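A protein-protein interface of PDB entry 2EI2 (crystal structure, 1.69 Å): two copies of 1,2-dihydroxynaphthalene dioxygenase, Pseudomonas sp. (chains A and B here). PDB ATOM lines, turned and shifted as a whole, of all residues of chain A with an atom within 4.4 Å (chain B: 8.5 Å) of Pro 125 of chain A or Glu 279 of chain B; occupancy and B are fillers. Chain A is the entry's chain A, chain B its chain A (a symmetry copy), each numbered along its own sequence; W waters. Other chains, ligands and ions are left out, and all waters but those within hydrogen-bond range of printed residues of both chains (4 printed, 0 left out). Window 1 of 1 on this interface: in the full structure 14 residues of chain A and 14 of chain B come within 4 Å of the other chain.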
ATOM      1  N   TRP A  51     -19.559 -32.561  12.230  1.00  0.00           N
ATOM      2  CA  TRP A  51     -18.313 -32.703  12.978  1.00  0.00           C
ATOM      3  C   TRP A  51     -18.138 -34.159  13.398  1.00  0.00           C
ATOM      4  O   TRP A  51     -19.116 -34.847  13.713  1.00  0.00           O
ATOM      5  CB  TRP A  51     -18.311 -31.811  14.229  1.00  0.00           C
ATOM      6  CG  TRP A  51     -18.046 -30.359  13.941  1.00  0.00           C
ATOM      7  CD1 TRP A  51     -18.508 -29.628  12.873  1.00  0.00           C
ATOM      8  CD2 TRP A  51     -17.284 -29.455  14.747  1.00  0.00           C
ATOM      9  NE1 TRP A  51     -18.068 -28.327  12.963  1.00  0.00           N
ATOM     10  CE2 TRP A  51     -17.320 -28.197  14.110  1.00  0.00           C
ATOM     11  CE3 TRP A  51     -16.565 -29.589  15.945  1.00  0.00           C
ATOM     12  CZ2 TRP A  51     -16.653 -27.094  14.615  1.00  0.00           C
ATOM     13  CZ3 TRP A  51     -15.938 -28.470  16.477  1.00  0.00           C
ATOM     14  CH2 TRP A  51     -15.972 -27.247  15.806  1.00  0.00           C
ATOM     15  N   ARG A  71     -13.127 -22.702  19.766  1.00  0.00           N
ATOM     16  CA  ARG A  71     -12.482 -22.673  18.443  1.00  0.00           C
ATOM     17  C   ARG A  71     -11.991 -21.282  18.055  1.00  0.00           C
ATOM     18  O   ARG A  71     -12.672 -20.286  18.334  1.00  0.00           O
ATOM     19  CB  ARG A  71     -13.488 -23.140  17.381  1.00  0.00           C
ATOM     20  CG  ARG A  71     -12.885 -23.359  16.002  1.00  0.00           C
ATOM     21  CD  ARG A  71     -14.022 -23.642  15.018  1.00  0.00           C
ATOM     22  NE  ARG A  71     -13.521 -23.950  13.684  1.00  0.00           N
ATOM     23  CZ  ARG A  71     -14.282 -24.136  12.608  1.00  0.00           C
ATOM     24  NH1 ARG A  71     -15.620 -24.070  12.672  1.00  0.00           N
ATOM     25  NH2 ARG A  71     -13.697 -24.434  11.448  1.00  0.00           N
ATOM     26  N   MET A 104      -8.592 -34.626  18.172  1.00  0.00           N
ATOM     27  CA  MET A 104      -8.856 -34.560  16.729  1.00  0.00           C
ATOM     28  C   MET A 104      -8.887 -33.138  16.188  1.00  0.00           C
ATOM     29  O   MET A 104      -9.804 -32.760  15.445  1.00  0.00           O
ATOM     30  CB  MET A 104     -10.126 -35.330  16.357  1.00  0.00           C
ATOM     31  CG  MET A 104      -9.976 -36.813  16.704  1.00  0.00           C
ATOM     32  SD  MET A 104     -11.477 -37.719  16.384  1.00  0.00           S
ATOM     33  CE  MET A 104     -11.309 -39.012  17.606  1.00  0.00           C
ATOM     34  N   PHE A 122      -8.489 -24.212  20.391  1.00  0.00           N
ATOM     35  CA  PHE A 122      -8.005 -25.040  19.294  1.00  0.00           C
ATOM     36  C   PHE A 122      -8.345 -24.426  17.947  1.00  0.00           C
ATOM     37  O   PHE A 122      -9.193 -23.538  17.853  1.00  0.00           O
ATOM     38  CB  PHE A 122      -8.639 -26.429  19.379  1.00  0.00           C
ATOM     39  CG  PHE A 122     -10.082 -26.466  18.965  1.00  0.00           C
ATOM     40  CD1 PHE A 122     -11.103 -26.188  19.878  1.00  0.00           C
ATOM     41  CD2 PHE A 122     -10.428 -26.790  17.648  1.00  0.00           C
ATOM     42  CE1 PHE A 122     -12.446 -26.229  19.483  1.00  0.00           C
ATOM     43  CE2 PHE A 122     -11.759 -26.820  17.241  1.00  0.00           C
ATOM     44  CZ  PHE A 122     -12.767 -26.544  18.147  1.00  0.00           C
ATOM     45  N   TRP A 123      -7.662 -24.904  16.912  1.00  0.00           N
ATOM     46  CA  TRP A 123      -8.074 -24.614  15.546  1.00  0.00           C
ATOM     47  C   TRP A 123      -8.086 -25.911  14.743  1.00  0.00           C
ATOM     48  O   TRP A 123      -7.361 -26.855  15.059  1.00  0.00           O
ATOM     49  CB  TRP A 123      -7.175 -23.542  14.909  1.00  0.00           C
ATOM     50  CG  TRP A 123      -5.777 -23.991  14.566  1.00  0.00           C
ATOM     51  CD1 TRP A 123      -4.680 -23.980  15.384  1.00  0.00           C
ATOM     52  CD2 TRP A 123      -5.325 -24.488  13.301  1.00  0.00           C
ATOM     53  NE1 TRP A 123      -3.582 -24.455  14.712  1.00  0.00           N
ATOM     54  CE2 TRP A 123      -3.951 -24.781  13.435  1.00  0.00           C
ATOM     55  CE3 TRP A 123      -5.954 -24.730  12.074  1.00  0.00           C
ATOM     56  CZ2 TRP A 123      -3.190 -25.296  12.391  1.00  0.00           C
ATOM     57  CZ3 TRP A 123      -5.188 -25.235  11.019  1.00  0.00           C
ATOM     58  CH2 TRP A 123      -3.818 -25.511  11.193  1.00  0.00           C
ATOM     59  N   GLY A 124      -8.917 -25.945  13.705  1.00  0.00           N
ATOM     60  CA  GLY A 124      -8.940 -27.076  12.779  1.00  0.00           C
ATOM     61  C   GLY A 124      -9.627 -28.326  13.289  1.00  0.00           C
ATOM     62  O   GLY A 124      -8.995 -29.367  13.436  1.00  0.00           O
ATOM     63  N   PRO A 125     -10.946 -28.263  13.493  1.00  0.00           N
ATOM     64  CA  PRO A 125     -11.673 -29.458  13.907  1.00  0.00           C
ATOM     65  C   PRO A 125     -11.759 -30.454  12.748  1.00  0.00           C
ATOM     66  O   PRO A 125     -11.678 -30.065  11.575  1.00  0.00           O
ATOM     67  CB  PRO A 125     -13.073 -28.915  14.210  1.00  0.00           C
ATOM     68  CG  PRO A 125     -13.210 -27.738  13.256  1.00  0.00           C
ATOM     69  CD  PRO A 125     -11.836 -27.103  13.299  1.00  0.00           C
ATOM     70  N   ARG A 126     -11.923 -31.728  13.085  1.00  0.00           N
ATOM     71  CA  ARG A 126     -12.185 -32.775  12.091  1.00  0.00           C
ATOM     72  C   ARG A 126     -13.674 -32.839  11.742  1.00  0.00           C
ATOM     73  O   ARG A 126     -14.528 -33.005  12.621  1.00  0.00           O
ATOM     74  CB  ARG A 126     -11.727 -34.137  12.635  1.00  0.00           C
ATOM     75  CG  ARG A 126     -12.069 -35.259  11.667  1.00  0.00           C
ATOM     76  CD  ARG A 126     -11.682 -36.611  12.252  1.00  0.00           C
ATOM     77  NE  ARG A 126     -12.432 -37.693  11.614  1.00  0.00           N
ATOM     78  CZ  ARG A 126     -12.135 -38.984  11.756  1.00  0.00           C
ATOM     79  NH1 ARG A 126     -11.082 -39.342  12.480  1.00  0.00           N
ATOM     80  NH2 ARG A 126     -12.875 -39.911  11.158  1.00  0.00           N
ATOM     81  N   ILE A 127     -13.975 -32.728  10.453  1.00  0.00           N
ATOM     82  CA  ILE A 127     -15.355 -32.727   9.950  1.00  0.00           C
ATOM     83  C   ILE A 127     -15.516 -33.961   9.073  1.00  0.00           C
ATOM     84  O   ILE A 127     -14.712 -34.181   8.143  1.00  0.00           O
ATOM     85  CB  ILE A 127     -15.637 -31.494   9.072  1.00  0.00           C
ATOM     86  CG1 ILE A 127     -15.197 -30.189   9.747  1.00  0.00           C
ATOM     87  CG2 ILE A 127     -17.126 -31.445   8.638  1.00  0.00           C
ATOM     88  CD1 ILE A 127     -15.814 -29.911  11.042  1.00  0.00           C
ATOM     89  N   GLY B 174      -5.285 -20.273   4.426  1.00  0.00           N
ATOM     90  CA  GLY B 174      -5.648 -21.686   4.440  1.00  0.00           C
ATOM     91  C   GLY B 174      -4.531 -22.551   4.986  1.00  0.00           C
ATOM     92  O   GLY B 174      -3.424 -22.080   5.243  1.00  0.00           O
ATOM     93  N   ASP B 175      -4.814 -23.834   5.165  1.00  0.00           N
ATOM     94  CA  ASP B 175      -3.846 -24.707   5.812  1.00  0.00           C
ATOM     95  C   ASP B 175      -4.183 -26.138   5.427  1.00  0.00           C
ATOM     96  O   ASP B 175      -4.864 -26.364   4.410  1.00  0.00           O
ATOM     97  CB  ASP B 175      -3.875 -24.494   7.342  1.00  0.00           C
ATOM     98  CG  ASP B 175      -2.507 -24.658   7.987  1.00  0.00           C
ATOM     99  OD1 ASP B 175      -1.923 -25.767   7.893  1.00  0.00           O
ATOM    100  OD2 ASP B 175      -2.014 -23.672   8.599  1.00  0.00           O
ATOM    101  N   VAL B 176      -3.699 -27.104   6.207  1.00  0.00           N
ATOM    102  CA  VAL B 176      -3.942 -28.514   5.897  1.00  0.00           C
ATOM    103  C   VAL B 176      -5.447 -28.757   5.984  1.00  0.00           C
ATOM    104  O   VAL B 176      -6.038 -28.488   7.032  1.00  0.00           O
ATOM    105  CB  VAL B 176      -3.239 -29.402   6.933  1.00  0.00           C
ATOM    106  CG1 VAL B 176      -3.708 -30.858   6.845  1.00  0.00           C
ATOM    107  CG2 VAL B 176      -1.724 -29.295   6.777  1.00  0.00           C
ATOM    108  N   GLU B 177      -6.065 -29.273   4.918  1.00  0.00           N
ATOM    109  CA  GLU B 177      -7.497 -29.632   4.971  1.00  0.00           C
ATOM    110  C   GLU B 177      -7.746 -31.123   4.785  1.00  0.00           C
ATOM    111  O   GLU B 177      -8.840 -31.610   5.067  1.00  0.00           O
ATOM    112  CB  GLU B 177      -8.316 -28.854   3.922  1.00  0.00           C
ATOM    113  CG  GLU B 177      -8.373 -27.375   4.255  1.00  0.00           C
ATOM    114  CD  GLU B 177      -9.095 -26.541   3.217  1.00  0.00           C
ATOM    115  OE1 GLU B 177      -9.491 -27.092   2.174  1.00  0.00           O
ATOM    116  OE2 GLU B 177      -9.227 -25.319   3.451  1.00  0.00           O
ATOM    117  N   TYR B 178      -6.753 -31.856   4.286  1.00  0.00           N
ATOM    118  CA  TYR B 178      -6.949 -33.284   4.113  1.00  0.00           C
ATOM    119  C   TYR B 178      -5.838 -34.056   4.768  1.00  0.00           C
ATOM    120  O   TYR B 178      -4.673 -33.758   4.530  1.00  0.00           O
ATOM    121  CB  TYR B 178      -6.984 -33.662   2.638  1.00  0.00           C
ATOM    122  CG  TYR B 178      -8.371 -33.875   2.060  1.00  0.00           C
ATOM    123  CD1 TYR B 178      -9.130 -32.814   1.622  1.00  0.00           C
ATOM    124  CD2 TYR B 178      -8.895 -35.156   1.926  1.00  0.00           C
ATOM    125  CE1 TYR B 178     -10.389 -33.014   1.077  1.00  0.00           C
ATOM    126  CE2 TYR B 178     -10.160 -35.377   1.377  1.00  0.00           C
ATOM    127  CZ  TYR B 178     -10.903 -34.300   0.957  1.00  0.00           C
ATOM    128  OH  TYR B 178     -12.160 -34.510   0.390  1.00  0.00           O
ATOM    129  N   ARG B 179      -6.206 -35.039   5.592  1.00  0.00           N
ATOM    130  CA  ARG B 179      -5.240 -35.992   6.151  1.00  0.00           C
ATOM    131  C   ARG B 179      -5.704 -37.369   5.705  1.00  0.00           C
ATOM    132  O   ARG B 179      -6.671 -37.920   6.248  1.00  0.00           O
ATOM    133  CB  ARG B 179      -5.152 -35.895   7.681  1.00  0.00           C
ATOM    134  CG  ARG B 179      -4.768 -34.492   8.183  1.00  0.00           C
ATOM    135  CD  ARG B 179      -4.384 -34.463   9.659  1.00  0.00           C
ATOM    136  NE  ARG B 179      -3.032 -34.957   9.863  1.00  0.00           N
ATOM    137  CZ  ARG B 179      -2.724 -36.065  10.530  1.00  0.00           C
ATOM    138  NH1 ARG B 179      -3.680 -36.798  11.084  1.00  0.00           N
ATOM    139  NH2 ARG B 179      -1.459 -36.438  10.648  1.00  0.00           N
ATOM    140  N   LEU B 190      -2.521 -32.533   2.667  1.00  0.00           N
ATOM    141  CA  LEU B 190      -2.569 -31.551   1.603  1.00  0.00           C
ATOM    142  C   LEU B 190      -3.122 -30.246   2.154  1.00  0.00           C
ATOM    143  O   LEU B 190      -4.081 -30.248   2.940  1.00  0.00           O
ATOM    144  CB  LEU B 190      -3.470 -32.020   0.452  1.00  0.00           C
ATOM    145  CG  LEU B 190      -2.887 -33.059  -0.502  1.00  0.00           C
ATOM    146  CD1 LEU B 190      -3.967 -33.467  -1.494  1.00  0.00           C
ATOM    147  CD2 LEU B 190      -1.673 -32.489  -1.227  1.00  0.00           C
ATOM    148  N   PHE B 192      -4.591 -26.228   1.364  1.00  0.00           N
ATOM    149  CA  PHE B 192      -5.403 -25.562   0.338  1.00  0.00           C
ATOM    150  C   PHE B 192      -5.557 -24.107   0.698  1.00  0.00           C
ATOM    151  O   PHE B 192      -5.964 -23.805   1.821  1.00  0.00           O
ATOM    152  CB  PHE B 192      -6.797 -26.196   0.277  1.00  0.00           C
ATOM    153  CG  PHE B 192      -6.761 -27.652  -0.113  1.00  0.00           C
ATOM    154  CD1 PHE B 192      -6.478 -28.629   0.838  1.00  0.00           C
ATOM    155  CD2 PHE B 192      -6.990 -28.049  -1.420  1.00  0.00           C
ATOM    156  CE1 PHE B 192      -6.434 -29.967   0.497  1.00  0.00           C
ATOM    157  CE2 PHE B 192      -6.956 -29.396  -1.772  1.00  0.00           C
ATOM    158  CZ  PHE B 192      -6.670 -30.357  -0.828  1.00  0.00           C
ATOM    159  N   ASP B 199     -13.233 -21.874  -3.566  1.00  0.00           N
ATOM    160  CA  ASP B 199     -12.817 -22.598  -2.364  1.00  0.00           C
ATOM    161  C   ASP B 199     -11.309 -22.580  -2.149  1.00  0.00           C
ATOM    162  O   ASP B 199     -10.818 -22.387  -1.021  1.00  0.00           O
ATOM    163  CB  ASP B 199     -13.292 -24.040  -2.374  1.00  0.00           C
ATOM    164  CG  ASP B 199     -12.775 -24.788  -1.174  1.00  0.00           C
ATOM    165  OD1 ASP B 199     -13.345 -24.558  -0.075  1.00  0.00           O
ATOM    166  OD2 ASP B 199     -11.757 -25.525  -1.295  1.00  0.00           O
ATOM    167  N   ALA B 248     -14.540 -33.130  -0.018  1.00  0.00           N
ATOM    168  CA  ALA B 248     -15.175 -32.596   1.181  1.00  0.00           C
ATOM    169  C   ALA B 248     -14.944 -31.102   1.372  1.00  0.00           C
ATOM    170  O   ALA B 248     -15.753 -30.441   2.014  1.00  0.00           O
ATOM    171  CB  ALA B 248     -14.698 -33.388   2.423  1.00  0.00           C
ATOM    172  N   ASN B 249     -13.845 -30.560   0.839  1.00  0.00           N
ATOM    173  CA  ASN B 249     -13.628 -29.113   0.980  1.00  0.00           C
ATOM    174  C   ASN B 249     -14.349 -28.274  -0.058  1.00  0.00           C
ATOM    175  O   ASN B 249     -15.215 -27.470   0.304  1.00  0.00           O
ATOM    176  CB  ASN B 249     -12.120 -28.741   1.087  1.00  0.00           C
ATOM    177  CG  ASN B 249     -11.246 -29.364  -0.011  1.00  0.00           C
ATOM    178  OD1 ASN B 249     -11.726 -30.058  -0.887  1.00  0.00           O
ATOM    179  ND2 ASN B 249      -9.925 -29.108   0.058  1.00  0.00           N
ATOM    180  N   LYS B 251     -16.470 -29.194  -2.443  1.00  0.00           N
ATOM    181  CA  LYS B 251     -17.860 -29.647  -2.611  1.00  0.00           C
ATOM    182  C   LYS B 251     -18.395 -29.628  -4.056  1.00  0.00           C
ATOM    183  O   LYS B 251     -19.608 -29.671  -4.280  1.00  0.00           O
ATOM    184  CB  LYS B 251     -18.796 -28.897  -1.641  1.00  0.00           C
ATOM    185  CG  LYS B 251     -18.499 -29.356  -0.174  1.00  0.00           C
ATOM    186  CD  LYS B 251     -19.189 -28.469   0.842  1.00  0.00           C
ATOM    187  CE  LYS B 251     -18.655 -28.751   2.235  1.00  0.00           C
ATOM    188  NZ  LYS B 251     -17.371 -28.015   2.480  1.00  0.00           N
ATOM    189  N   ILE B 275     -14.122 -20.556   2.851  1.00  0.00           N
ATOM    190  CA  ILE B 275     -14.333 -20.141   4.237  1.00  0.00           C
ATOM    191  C   ILE B 275     -13.022 -19.853   4.944  1.00  0.00           C
ATOM    192  O   ILE B 275     -12.024 -20.516   4.690  1.00  0.00           O
ATOM    193  CB  ILE B 275     -15.174 -21.149   5.059  1.00  0.00           C
ATOM    194  CG1 ILE B 275     -14.474 -22.500   5.195  1.00  0.00           C
ATOM    195  CG2 ILE B 275     -16.582 -21.316   4.446  1.00  0.00           C
ATOM    196  CD1 ILE B 275     -15.200 -23.412   6.177  1.00  0.00           C
ATOM    197  N   ASP B 276     -13.019 -18.848   5.823  1.00  0.00           N
ATOM    198  CA  ASP B 276     -11.781 -18.489   6.504  1.00  0.00           C
ATOM    199  C   ASP B 276     -11.500 -19.409   7.689  1.00  0.00           C
ATOM    200  O   ASP B 276     -10.350 -19.484   8.146  1.00  0.00           O
ATOM    201  CB  ASP B 276     -11.800 -17.028   6.974  1.00  0.00           C
ATOM    202  CG  ASP B 276     -11.504 -16.028   5.851  1.00  0.00           C
ATOM    203  OD1 ASP B 276     -10.939 -16.412   4.800  1.00  0.00           O
ATOM    204  OD2 ASP B 276     -11.821 -14.836   6.036  1.00  0.00           O
ATOM    205  N   GLU B 277     -12.531 -20.114   8.171  1.00  0.00           N
ATOM    206  CA  GLU B 277     -12.377 -20.996   9.347  1.00  0.00           C
ATOM    207  C   GLU B 277     -11.768 -22.347   8.944  1.00  0.00           C
ATOM    208  O   GLU B 277     -12.351 -23.104   8.166  1.00  0.00           O
ATOM    209  CB  GLU B 277     -13.729 -21.162  10.061  1.00  0.00           C
ATOM    210  CG  GLU B 277     -14.362 -19.821  10.515  1.00  0.00           C
ATOM    211  CD  GLU B 277     -14.945 -18.975   9.379  1.00  0.00           C
ATOM    212  OE1 GLU B 277     -15.357 -19.524   8.335  1.00  0.00           O
ATOM    213  OE2 GLU B 277     -14.999 -17.739   9.551  1.00  0.00           O
ATOM    214  N   ALA B 278     -10.574 -22.635   9.448  1.00  0.00           N
ATOM    215  CA  ALA B 278      -9.877 -23.863   9.048  1.00  0.00           C
ATOM    216  C   ALA B 278     -10.561 -25.113   9.598  1.00  0.00           C
ATOM    217  O   ALA B 278     -10.879 -25.201  10.786  1.00  0.00           O
ATOM    218  CB  ALA B 278      -8.407 -23.814   9.529  1.00  0.00           C
ATOM    219  N   GLU B 279     -10.757 -26.104   8.743  1.00  0.00           N
ATOM    220  CA  GLU B 279     -11.071 -27.429   9.245  1.00  0.00           C
ATOM    221  C   GLU B 279     -10.428 -28.488   8.369  1.00  0.00           C
ATOM    222  O   GLU B 279      -9.871 -28.159   7.324  1.00  0.00           O
ATOM    223  CB  GLU B 279     -12.558 -27.638   9.279  1.00  0.00           C
ATOM    224  CG  GLU B 279     -13.180 -27.543   7.938  1.00  0.00           C
ATOM    225  CD  GLU B 279     -14.624 -27.079   8.010  1.00  0.00           C
ATOM    226  OE1 GLU B 279     -14.970 -26.364   8.977  1.00  0.00           O
ATOM    227  OE2 GLU B 279     -15.407 -27.443   7.097  1.00  0.00           O
ATOM    228  N   TYR B 280     -10.489 -29.745   8.801  1.00  0.00           N
ATOM    229  CA  TYR B 280      -9.934 -30.809   7.970  1.00  0.00           C
ATOM    230  C   TYR B 280     -10.824 -32.026   7.870  1.00  0.00           C
ATOM    231  O   TYR B 280     -11.766 -32.189   8.656  1.00  0.00           O
ATOM    232  CB  TYR B 280      -8.528 -31.218   8.419  1.00  0.00           C
ATOM    233  CG  TYR B 280      -8.465 -32.107   9.632  1.00  0.00           C
ATOM    234  CD1 TYR B 280      -8.573 -31.583  10.929  1.00  0.00           C
ATOM    235  CD2 TYR B 280      -8.245 -33.476   9.501  1.00  0.00           C
ATOM    236  CE1 TYR B 280      -8.480 -32.426  12.065  1.00  0.00           C
ATOM    237  CE2 TYR B 280      -8.157 -34.320  10.601  1.00  0.00           C
ATOM    238  CZ  TYR B 280      -8.270 -33.797  11.885  1.00  0.00           C
ATOM    239  OH  TYR B 280      -8.177 -34.663  12.968  1.00  0.00           O
ATOM    240  N   TYR B 281     -10.530 -32.848   6.862  1.00  0.00           N
ATOM    241  CA  TYR B 281     -11.339 -34.009   6.524  1.00  0.00           C
ATOM    242  C   TYR B 281     -10.418 -35.200   6.307  1.00  0.00           C
ATOM    243  O   TYR B 281      -9.227 -35.036   6.036  1.00  0.00           O
ATOM    244  CB  TYR B 281     -12.072 -33.730   5.202  1.00  0.00           C
ATOM    245  CG  TYR B 281     -12.660 -32.331   5.127  1.00  0.00           C
ATOM    246  CD1 TYR B 281     -11.960 -31.289   4.522  1.00  0.00           C
ATOM    247  CD2 TYR B 281     -13.889 -32.051   5.702  1.00  0.00           C
ATOM    248  CE1 TYR B 281     -12.493 -29.990   4.469  1.00  0.00           C
ATOM    249  CE2 TYR B 281     -14.430 -30.757   5.654  1.00  0.00           C
ATOM    250  CZ  TYR B 281     -13.722 -29.746   5.042  1.00  0.00           C
ATOM    251  OH  TYR B 281     -14.275 -28.476   5.005  1.00  0.00           O
ATOM    252  N   VAL B 282     -10.963 -36.409   6.415  1.00  0.00           N
ATOM    253  CA  VAL B 282     -10.148 -37.607   6.136  1.00  0.00           C
ATOM    254  C   VAL B 282     -10.676 -38.432   4.958  1.00  0.00           C
ATOM    255  O   VAL B 282     -10.254 -39.569   4.753  1.00  0.00           O
ATOM    256  CB  VAL B 282      -9.971 -38.502   7.381  1.00  0.00           C
ATOM    257  CG1 VAL B 282      -9.346 -37.700   8.511  1.00  0.00           C
ATOM    258  CG2 VAL B 282     -11.318 -39.107   7.823  1.00  0.00           C
HETATM  259  O   HOH W   1     -13.679 -36.673   7.206  1.00  0.00           O
HETATM  260  O   HOH W   2      -8.187 -37.660  12.851  1.00  0.00           O
HETATM  261  O   HOH W   3     -16.298 -24.213   9.804  1.00  0.00           O
HETATM  262  O   HOH W   4     -10.631 -23.601  13.205  1.00  0.00           O
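The side-chain carboxylate (OE1) of Glu 279 of chain B lies within salt-bridge range of the guanidinium group (NH2) of Arg 71 of chain A, 3.4 Å away. The backbone carbonyl oxygen of Pro 125 of chain A sits at hydrogen-bond distance from the backbone NH of Tyr 280 of chain B (3.0 Å). The backbone NH (N) of Ile 127 of chain A sits at hydrogen-bond distance from the backbone carbonyl oxygen (O) of Tyr 280 of chain B (2.9 Å). The guanidinium group of Arg 71 of chain A sits at hydrogen-bond distance from the backbone carbonyl oxygen of Ala 278 of chain B, 3.0 Å away.
No position is printed for both chains.
Arg 71 of chain A touches Glu 277 of chain B (NH2 to CB, 3.6 Å). Met 104 of chain A touches Tyr 280 of chain B (O to OH, 3.5 Å). Trp 123 of chain A touches Asp 175 of chain B. Gly 124 of chain A touches Ala 278 of chain B. CD1 of Tyr 280 of chain B touches O of Gly 124 of chain A, 3.4 Å away. Glu 279 of chain B touches Pro 125 of chain A. Tyr 280 of chain B touches Arg 126 of chain A. Val 282 of chain B touches Arg 126 of chain A. CG1 of Ile 127 of chain A touches CD of Glu 279 of chain B, at 3.6 Å. O of Ile 127 of chain A touches CD2 of Tyr 281 of chain B (3.3 Å).
Of the printed residues of chain B, Arg 71 of chain A touches Glu 277, Ala 278 and Glu 279. Of the printed residues of chain B, Trp 123 of chain A touches Asp 175 and Ala 278. Gly 124 of chain A touches just these residues of chain B: Ala 278 and Tyr 280. Pro 125 of chain A touches just these residues of chain B: Ala 278 (3.3 Å), Glu 279 (3.5 Å) and Tyr 280 (3.0 Å). Printed residues of chain B within 4 Å of Ile 127 of chain A: Glu 279 (3.6 Å), Tyr 280 (2.9 Å) and Tyr 281 (3.3 Å). Of the printed residues of chain A, Glu 277 of chain B touches Arg 71. The nearest residue of chain B that does not touch Pro 125 of chain A is Tyr 281 of chain B (5.6 Å).
Water W3 bridges OE1 of Glu 279 of chain B and NH1 of Arg 71 of chain A. Water W1 bridges N of Val 282 of chain B and O of Ile 127 of chain A. Water W4 lies within hydrogen-bond range of the backbone carbonyl oxygen (O) of Ala 278 of chain B (2.9 Å), the backbone NH (N) of Gly 124 of chain A (2.9 Å) and the guanidinium group (NE) of Arg 71 of chain A (3.0 Å). Water W2 lies within hydrogen-bond range of the side-chain hydroxyl of Tyr 280 of chain B and the guanidinium group of Arg 126 of chain A.
The backbone carbonyl oxygen of Met 104 of chain A is in hydrogen-bond range of the backbone NH of Arg 126 of chain A (3.3 Å). The backbone carbonyl oxygen (O) of Asp 175 of chain B is in hydrogen-bond range of the backbone NH (N) of Phe 192 of chain B (3.1 Å). O of Glu 177 of chain B sits at hydrogen-bond distance from N of Tyr 281 of chain B. The side-chain hydroxyl of Tyr 281 of chain B sits at hydrogen-bond distance from the side-chain carboxylate of Glu 279 of chain B (2.6 Å). The backbone carbonyl oxygen of Tyr 281 of chain B is in hydrogen-bond range of the backbone NH of Arg 179 of chain B (3.1 Å).
Hydrophobic or aromatic side chains of chain B that line the printed part of chain A: Ala 278, Tyr 280, Tyr 281 and Val 282. Hydrophobic or aromatic side chains of chain A within 4 Å of the printed part of chain B: Met 104, Trp 123, Pro 125 and Ile 127. Among the printed residues, 16 pairs touch across the chains.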
